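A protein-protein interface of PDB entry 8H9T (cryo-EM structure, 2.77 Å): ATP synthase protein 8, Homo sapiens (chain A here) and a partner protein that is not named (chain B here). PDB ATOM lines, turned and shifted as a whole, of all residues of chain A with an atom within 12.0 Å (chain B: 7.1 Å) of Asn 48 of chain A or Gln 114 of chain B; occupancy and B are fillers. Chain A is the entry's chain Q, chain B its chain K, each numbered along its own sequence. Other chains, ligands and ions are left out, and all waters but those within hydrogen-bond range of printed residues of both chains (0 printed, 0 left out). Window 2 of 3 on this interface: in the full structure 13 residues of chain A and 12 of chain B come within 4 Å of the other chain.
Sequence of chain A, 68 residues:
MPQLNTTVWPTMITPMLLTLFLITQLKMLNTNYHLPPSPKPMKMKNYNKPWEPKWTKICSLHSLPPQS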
ATOM      1  N   MET A  44      -1.060  16.013  34.355  1.00  0.00           N
ATOM      2  CA  MET A  44      -1.738  15.094  33.445  1.00  0.00           C
ATOM      3  C   MET A  44      -0.725  14.585  32.432  1.00  0.00           C
ATOM      4  O   MET A  44      -0.437  15.249  31.434  1.00  0.00           O
ATOM      5  CB  MET A  44      -2.921  15.761  32.755  1.00  0.00           C
ATOM      6  CG  MET A  44      -3.970  14.776  32.240  1.00  0.00           C
ATOM      7  SD  MET A  44      -3.454  13.804  30.807  1.00  0.00           S
ATOM      8  CE  MET A  44      -3.059  15.096  29.632  1.00  0.00           C
ATOM      9  N   LYS A  45      -0.179  13.408  32.693  1.00  0.00           N
ATOM     10  CA  LYS A  45       0.487  12.635  31.655  1.00  0.00           C
ATOM     11  C   LYS A  45      -0.148  11.254  31.691  1.00  0.00           C
ATOM     12  O   LYS A  45       0.203  10.404  32.510  1.00  0.00           O
ATOM     13  CB  LYS A  45       1.995  12.584  31.852  1.00  0.00           C
ATOM     14  CG  LYS A  45       2.693  11.919  30.684  1.00  0.00           C
ATOM     15  CD  LYS A  45       2.287  12.611  29.393  1.00  0.00           C
ATOM     16  CE  LYS A  45       2.857  11.921  28.172  1.00  0.00           C
ATOM     17  NZ  LYS A  45       2.243  12.464  26.930  1.00  0.00           N
ATOM     18  N   ASN A  46      -1.112  11.042  30.800  1.00  0.00           N
ATOM     19  CA  ASN A  46      -1.779   9.754  30.684  1.00  0.00           C
ATOM     20  C   ASN A  46      -1.061   8.913  29.636  1.00  0.00           C
ATOM     21  O   ASN A  46      -0.353   7.967  29.988  1.00  0.00           O
ATOM     22  CB  ASN A  46      -3.247  10.019  30.319  1.00  0.00           C
ATOM     23  CG  ASN A  46      -3.972   8.808  29.753  1.00  0.00           C
ATOM     24  OD1 ASN A  46      -3.488   7.678  29.796  1.00  0.00           O
ATOM     25  ND2 ASN A  46      -5.160   9.053  29.210  1.00  0.00           N
ATOM     26  N   TYR A  47      -1.230   9.245  28.359  1.00  0.00           N
ATOM     27  CA  TYR A  47      -0.372   8.919  27.227  1.00  0.00           C
ATOM     28  C   TYR A  47      -1.164   9.349  26.006  1.00  0.00           C
ATOM     29  O   TYR A  47      -2.298   9.817  26.141  1.00  0.00           O
ATOM     30  CB  TYR A  47       0.014   7.438  27.145  1.00  0.00           C
ATOM     31  CG  TYR A  47       1.120   7.179  26.141  1.00  0.00           C
ATOM     32  CD1 TYR A  47       2.260   7.969  26.125  1.00  0.00           C
ATOM     33  CD2 TYR A  47       1.021   6.156  25.208  1.00  0.00           C
ATOM     34  CE1 TYR A  47       3.268   7.748  25.212  1.00  0.00           C
ATOM     35  CE2 TYR A  47       2.024   5.929  24.290  1.00  0.00           C
ATOM     36  CZ  TYR A  47       3.145   6.728  24.297  1.00  0.00           C
ATOM     37  OH  TYR A  47       4.150   6.505  23.388  1.00  0.00           O
ATOM     38  N   ASN A  48      -0.603   9.202  24.815  1.00  0.00           N
ATOM     39  CA  ASN A  48      -1.494   9.060  23.675  1.00  0.00           C
ATOM     40  C   ASN A  48      -2.022   7.632  23.672  1.00  0.00           C
ATOM     41  O   ASN A  48      -1.782   6.871  24.613  1.00  0.00           O
ATOM     42  CB  ASN A  48      -0.792   9.388  22.360  1.00  0.00           C
ATOM     43  CG  ASN A  48      -1.772   9.715  21.253  1.00  0.00           C
ATOM     44  OD1 ASN A  48      -2.543  10.671  21.353  1.00  0.00           O
ATOM     45  ND2 ASN A  48      -1.763   8.910  20.198  1.00  0.00           N
ATOM     46  N   LYS A  49      -2.752   7.260  22.644  1.00  0.00           N
ATOM     47  CA  LYS A  49      -3.153   5.869  22.522  1.00  0.00           C
ATOM     48  C   LYS A  49      -1.951   5.097  21.993  1.00  0.00           C
ATOM     49  O   LYS A  49      -0.916   5.712  21.707  1.00  0.00           O
ATOM     50  CB  LYS A  49      -4.373   5.754  21.612  1.00  0.00           C
ATOM     51  CG  LYS A  49      -5.683   5.821  22.372  1.00  0.00           C
ATOM     52  CD  LYS A  49      -5.893   7.195  22.984  1.00  0.00           C
ATOM     53  CE  LYS A  49      -5.838   8.279  21.921  1.00  0.00           C
ATOM     54  NZ  LYS A  49      -6.057   9.634  22.482  1.00  0.00           N
ATOM     55  N   PRO A  50      -2.014   3.767  21.879  1.00  0.00           N
ATOM     56  CA  PRO A  50      -0.884   3.043  21.277  1.00  0.00           C
ATOM     57  C   PRO A  50      -0.480   3.590  19.928  1.00  0.00           C
ATOM     58  O   PRO A  50       0.698   3.499  19.557  1.00  0.00           O
ATOM     59  CB  PRO A  50      -1.405   1.603  21.169  1.00  0.00           C
ATOM     60  CG  PRO A  50      -2.883   1.698  21.392  1.00  0.00           C
ATOM     61  CD  PRO A  50      -3.047   2.830  22.344  1.00  0.00           C
ATOM     62  N   TRP A  51      -1.422   4.149  19.179  1.00  0.00           N
ATOM     63  CA  TRP A  51      -1.096   4.889  17.973  1.00  0.00           C
ATOM     64  C   TRP A  51      -0.817   6.349  18.317  1.00  0.00           C
ATOM     65  O   TRP A  51      -1.355   6.881  19.287  1.00  0.00           O
ATOM     66  CB  TRP A  51      -2.226   4.795  16.956  1.00  0.00           C
ATOM     67  CG  TRP A  51      -3.573   5.102  17.525  1.00  0.00           C
ATOM     68  CD1 TRP A  51      -4.505   4.203  17.944  1.00  0.00           C
ATOM     69  CD2 TRP A  51      -4.142   6.400  17.740  1.00  0.00           C
ATOM     70  NE1 TRP A  51      -5.620   4.857  18.404  1.00  0.00           N
ATOM     71  CE2 TRP A  51      -5.423   6.207  18.289  1.00  0.00           C
ATOM     72  CE3 TRP A  51      -3.695   7.703  17.518  1.00  0.00           C
ATOM     73  CZ2 TRP A  51      -6.257   7.264  18.621  1.00  0.00           C
ATOM     74  CZ3 TRP A  51      -4.522   8.749  17.850  1.00  0.00           C
ATOM     75  CH2 TRP A  51      -5.789   8.525  18.396  1.00  0.00           C
ATOM     76  N   ILE B 108     -10.330  15.197  33.391  1.00  0.00           N
ATOM     77  CA  ILE B 108     -11.490  14.442  32.917  1.00  0.00           C
ATOM     78  C   ILE B 108     -11.799  14.792  31.467  1.00  0.00           C
ATOM     79  O   ILE B 108     -12.003  13.910  30.623  1.00  0.00           O
ATOM     80  CB  ILE B 108     -12.706  14.704  33.818  1.00  0.00           C
ATOM     81  CG1 ILE B 108     -12.565  13.958  35.138  1.00  0.00           C
ATOM     82  CG2 ILE B 108     -13.976  14.281  33.125  1.00  0.00           C
ATOM     83  CD1 ILE B 108     -13.742  14.159  36.051  1.00  0.00           C
ATOM     84  N   ASP B 109     -11.860  16.086  31.163  1.00  0.00           N
ATOM     85  CA  ASP B 109     -12.207  16.492  29.808  1.00  0.00           C
ATOM     86  C   ASP B 109     -11.149  16.055  28.809  1.00  0.00           C
ATOM     87  O   ASP B 109     -11.481  15.687  27.675  1.00  0.00           O
ATOM     88  CB  ASP B 109     -12.419  18.000  29.752  1.00  0.00           C
ATOM     89  CG  ASP B 109     -13.668  18.434  30.493  1.00  0.00           C
ATOM     90  OD1 ASP B 109     -14.536  17.573  30.747  1.00  0.00           O
ATOM     91  OD2 ASP B 109     -13.784  19.632  30.825  1.00  0.00           O
ATOM     92  N   THR B 110      -9.880  16.068  29.211  1.00  0.00           N
ATOM     93  CA  THR B 110      -8.839  15.561  28.331  1.00  0.00           C
ATOM     94  C   THR B 110      -9.030  14.077  28.059  1.00  0.00           C
ATOM     95  O   THR B 110      -8.884  13.626  26.916  1.00  0.00           O
ATOM     96  CB  THR B 110      -7.469  15.828  28.939  1.00  0.00           C
ATOM     97  OG1 THR B 110      -7.279  17.241  29.060  1.00  0.00           O
ATOM     98  CG2 THR B 110      -6.385  15.254  28.057  1.00  0.00           C
ATOM     99  N   GLU B 111      -9.362  13.302  29.093  1.00  0.00           N
ATOM    100  CA  GLU B 111      -9.651  11.888  28.875  1.00  0.00           C
ATOM    101  C   GLU B 111     -10.794  11.709  27.886  1.00  0.00           C
ATOM    102  O   GLU B 111     -10.725  10.861  26.988  1.00  0.00           O
ATOM    103  CB  GLU B 111      -9.981  11.206  30.197  1.00  0.00           C
ATOM    104  CG  GLU B 111      -8.823  11.169  31.154  1.00  0.00           C
ATOM    105  CD  GLU B 111      -7.716  10.270  30.675  1.00  0.00           C
ATOM    106  OE1 GLU B 111      -7.963   9.058  30.524  1.00  0.00           O
ATOM    107  OE2 GLU B 111      -6.599  10.774  30.442  1.00  0.00           O
ATOM    108  N   LYS B 112     -11.850  12.506  28.030  1.00  0.00           N
ATOM    109  CA  LYS B 112     -12.989  12.378  27.125  1.00  0.00           C
ATOM    110  C   LYS B 112     -12.590  12.691  25.687  1.00  0.00           C
ATOM    111  O   LYS B 112     -13.023  12.009  24.748  1.00  0.00           O
ATOM    112  CB  LYS B 112     -14.122  13.291  27.579  1.00  0.00           C
ATOM    113  CG  LYS B 112     -14.819  12.813  28.829  1.00  0.00           C
ATOM    114  CD  LYS B 112     -16.217  13.378  28.913  1.00  0.00           C
ATOM    115  CE  LYS B 112     -16.878  12.991  30.217  1.00  0.00           C
ATOM    116  NZ  LYS B 112     -16.714  11.540  30.493  1.00  0.00           N
ATOM    117  N   SER B 113     -11.771  13.721  25.491  1.00  0.00           N
ATOM    118  CA  SER B 113     -11.335  14.050  24.139  1.00  0.00           C
ATOM    119  C   SER B 113     -10.496  12.924  23.551  1.00  0.00           C
ATOM    120  O   SER B 113     -10.629  12.583  22.367  1.00  0.00           O
ATOM    121  CB  SER B 113     -10.551  15.358  24.141  1.00  0.00           C
ATOM    122  OG  SER B 113      -9.322  15.202  24.823  1.00  0.00           O
ATOM    123  N   GLN B 114      -9.615  12.337  24.366  1.00  0.00           N
ATOM    124  CA  GLN B 114      -8.851  11.187  23.895  1.00  0.00           C
ATOM    125  C   GLN B 114      -9.780  10.057  23.484  1.00  0.00           C
ATOM    126  O   GLN B 114      -9.544   9.377  22.475  1.00  0.00           O
ATOM    127  CB  GLN B 114      -7.886  10.708  24.973  1.00  0.00           C
ATOM    128  CG  GLN B 114      -6.940  11.769  25.475  1.00  0.00           C
ATOM    129  CD  GLN B 114      -6.182  12.443  24.365  1.00  0.00           C
ATOM    130  OE1 GLN B 114      -6.602  13.479  23.854  1.00  0.00           O
ATOM    131  NE2 GLN B 114      -5.047  11.869  23.991  1.00  0.00           N
ATOM    132  N   GLN B 115     -10.844   9.844  24.254  1.00  0.00           N
ATOM    133  CA  GLN B 115     -11.816   8.818  23.900  1.00  0.00           C
ATOM    134  C   GLN B 115     -12.461   9.106  22.552  1.00  0.00           C
ATOM    135  O   GLN B 115     -12.622   8.199  21.730  1.00  0.00           O
ATOM    136  CB  GLN B 115     -12.878   8.709  24.981  1.00  0.00           C
ATOM    137  CG  GLN B 115     -12.314   8.302  26.306  1.00  0.00           C
ATOM    138  CD  GLN B 115     -13.376   7.819  27.250  1.00  0.00           C
ATOM    139  OE1 GLN B 115     -13.119   7.619  28.431  1.00  0.00           O
ATOM    140  NE2 GLN B 115     -14.582   7.622  26.735  1.00  0.00           N
ATOM    141  N   ALA B 116     -12.838  10.358  22.309  1.00  0.00           N
ATOM    142  CA  ALA B 116     -13.458  10.694  21.029  1.00  0.00           C
ATOM    143  C   ALA B 116     -12.506  10.434  19.865  1.00  0.00           C
ATOM    144  O   ALA B 116     -12.903   9.868  18.835  1.00  0.00           O
ATOM    145  CB  ALA B 116     -13.913  12.150  21.030  1.00  0.00           C
ATOM    146  N   LEU B 117     -11.248  10.854  20.004  1.00  0.00           N
ATOM    147  CA  LEU B 117     -10.279  10.616  18.938  1.00  0.00           C
ATOM    148  C   LEU B 117     -10.130   9.126  18.666  1.00  0.00           C
ATOM    149  O   LEU B 117     -10.201   8.671  17.511  1.00  0.00           O
ATOM    150  CB  LEU B 117      -8.926  11.217  19.307  1.00  0.00           C
ATOM    151  CG  LEU B 117      -8.878  12.698  19.659  1.00  0.00           C
ATOM    152  CD1 LEU B 117      -7.444  13.190  19.646  1.00  0.00           C
ATOM    153  CD2 LEU B 117      -9.728  13.493  18.696  1.00  0.00           C
ATOM    154  N   VAL B 118      -9.933   8.345  19.724  1.00  0.00           N
ATOM    155  CA  VAL B 118      -9.722   6.930  19.512  1.00  0.00           C
ATOM    156  C   VAL B 118     -10.997   6.247  19.044  1.00  0.00           C
ATOM    157  O   VAL B 118     -10.948   5.133  18.516  1.00  0.00           O
ATOM    158  CB  VAL B 118      -9.173   6.290  20.789  1.00  0.00           C
ATOM    159  CG1 VAL B 118     -10.278   6.069  21.795  1.00  0.00           C
ATOM    160  CG2 VAL B 118      -8.526   5.028  20.439  1.00  0.00           C
ATOM    161  N   GLN B 119     -12.146   6.892  19.217  1.00  0.00           N
ATOM    162  CA  GLN B 119     -13.354   6.416  18.562  1.00  0.00           C
ATOM    163  C   GLN B 119     -13.261   6.620  17.057  1.00  0.00           C
ATOM    164  O   GLN B 119     -13.505   5.695  16.274  1.00  0.00           O
ATOM    165  CB  GLN B 119     -14.570   7.142  19.132  1.00  0.00           C
ATOM    166  CG  GLN B 119     -15.887   6.676  18.569  1.00  0.00           C
ATOM    167  CD  GLN B 119     -16.095   5.194  18.766  1.00  0.00           C
ATOM    168  OE1 GLN B 119     -15.763   4.643  19.815  1.00  0.00           O
ATOM    169  NE2 GLN B 119     -16.646   4.537  17.755  1.00  0.00           N
ATOM    170  N   LYS B 120     -12.888   7.830  16.636  1.00  0.00           N
ATOM    171  CA  LYS B 120     -12.774   8.141  15.212  1.00  0.00           C
ATOM    172  C   LYS B 120     -11.657   7.379  14.516  1.00  0.00           C
ATOM    173  O   LYS B 120     -11.543   7.468  13.293  1.00  0.00           O
ATOM    174  CB  LYS B 120     -12.544   9.636  15.011  1.00  0.00           C
ATOM    175  CG  LYS B 120     -13.802  10.469  15.053  1.00  0.00           C
ATOM    176  CD  LYS B 120     -13.465  11.942  14.971  1.00  0.00           C
ATOM    177  CE  LYS B 120     -14.688  12.798  15.221  1.00  0.00           C
ATOM    178  NZ  LYS B 120     -14.311  14.209  15.485  1.00  0.00           N
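The side-chain carboxylate (OE2) of Glu 111 of chain B is in hydrogen-bond range of the side-chain amide nitrogen (ND2) of Asn 46 of chain A, 2.6 Å away. NE2 of Gln 114 of chain B lies close to NZ of Lys 49 of chain A (2.9 Å).
Of the printed residues of chain B, Met 44 of chain A touches Thr 110. Of the printed residues of chain B, Asn 46 of chain A touches Glu 111 (2.6 Å). Of the printed residues of chain B, Lys 49 of chain A touches Gln 114 and Val 118. Printed residues of chain B within 4 Å of Trp 51 of chain A: Val 118 (3.6 Å). Glu 111 of chain B touches one residue of chain A. Printed residues of chain A within 4 Å of Gln 114 of chain B: Asn 48 (3.8 Å) and Lys 49 (2.9 Å). No residue of chain A comes within 4 Å of Gln 115 of chain B. No residue of chain A comes within 4 Å of Ala 116 of chain B. Leu 117 of chain B touches none of the printed residues of chain A. The nearest printed residue of chain B that does not touch Asn 46 of chain A is Gln 114 of chain B (4.9 Å).
The side-chain amide oxygen (OE1) of Gln 114 of chain B lies within hydrogen-bond range of the side-chain hydroxyl (OG) of Ser 113 of chain B, 3.4 Å away. OG of Ser 113 of chain B lies within hydrogen-bond range of O of Thr 110 of chain B. The backbone NH (N) of Asn 46 of chain A sits at hydrogen-bond distance from the side-chain sulfur (SD) of Met 44 of chain A, at 3.6 Å.
Of the 8 printed residues of chain A, 5 touch a printed residue of chain B. Hydrophobic or aromatic side chains of chain B within 4 Å of the printed part of chain A: Val 118. Among the printed residues, 6 pairs touch across the chains.
Among the printed residues, pairs that only touch across the chains: Met 44 of chain A with Thr 110 of chain B (3.7 Å), Asn 48 of chain A with Gln 114 of chain B (3.8 Å), Lys 49 of chain A with Val 118 of chain B (3.5 Å) and Trp 51 of chain A with Val 118 of chain B (3.6 Å).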
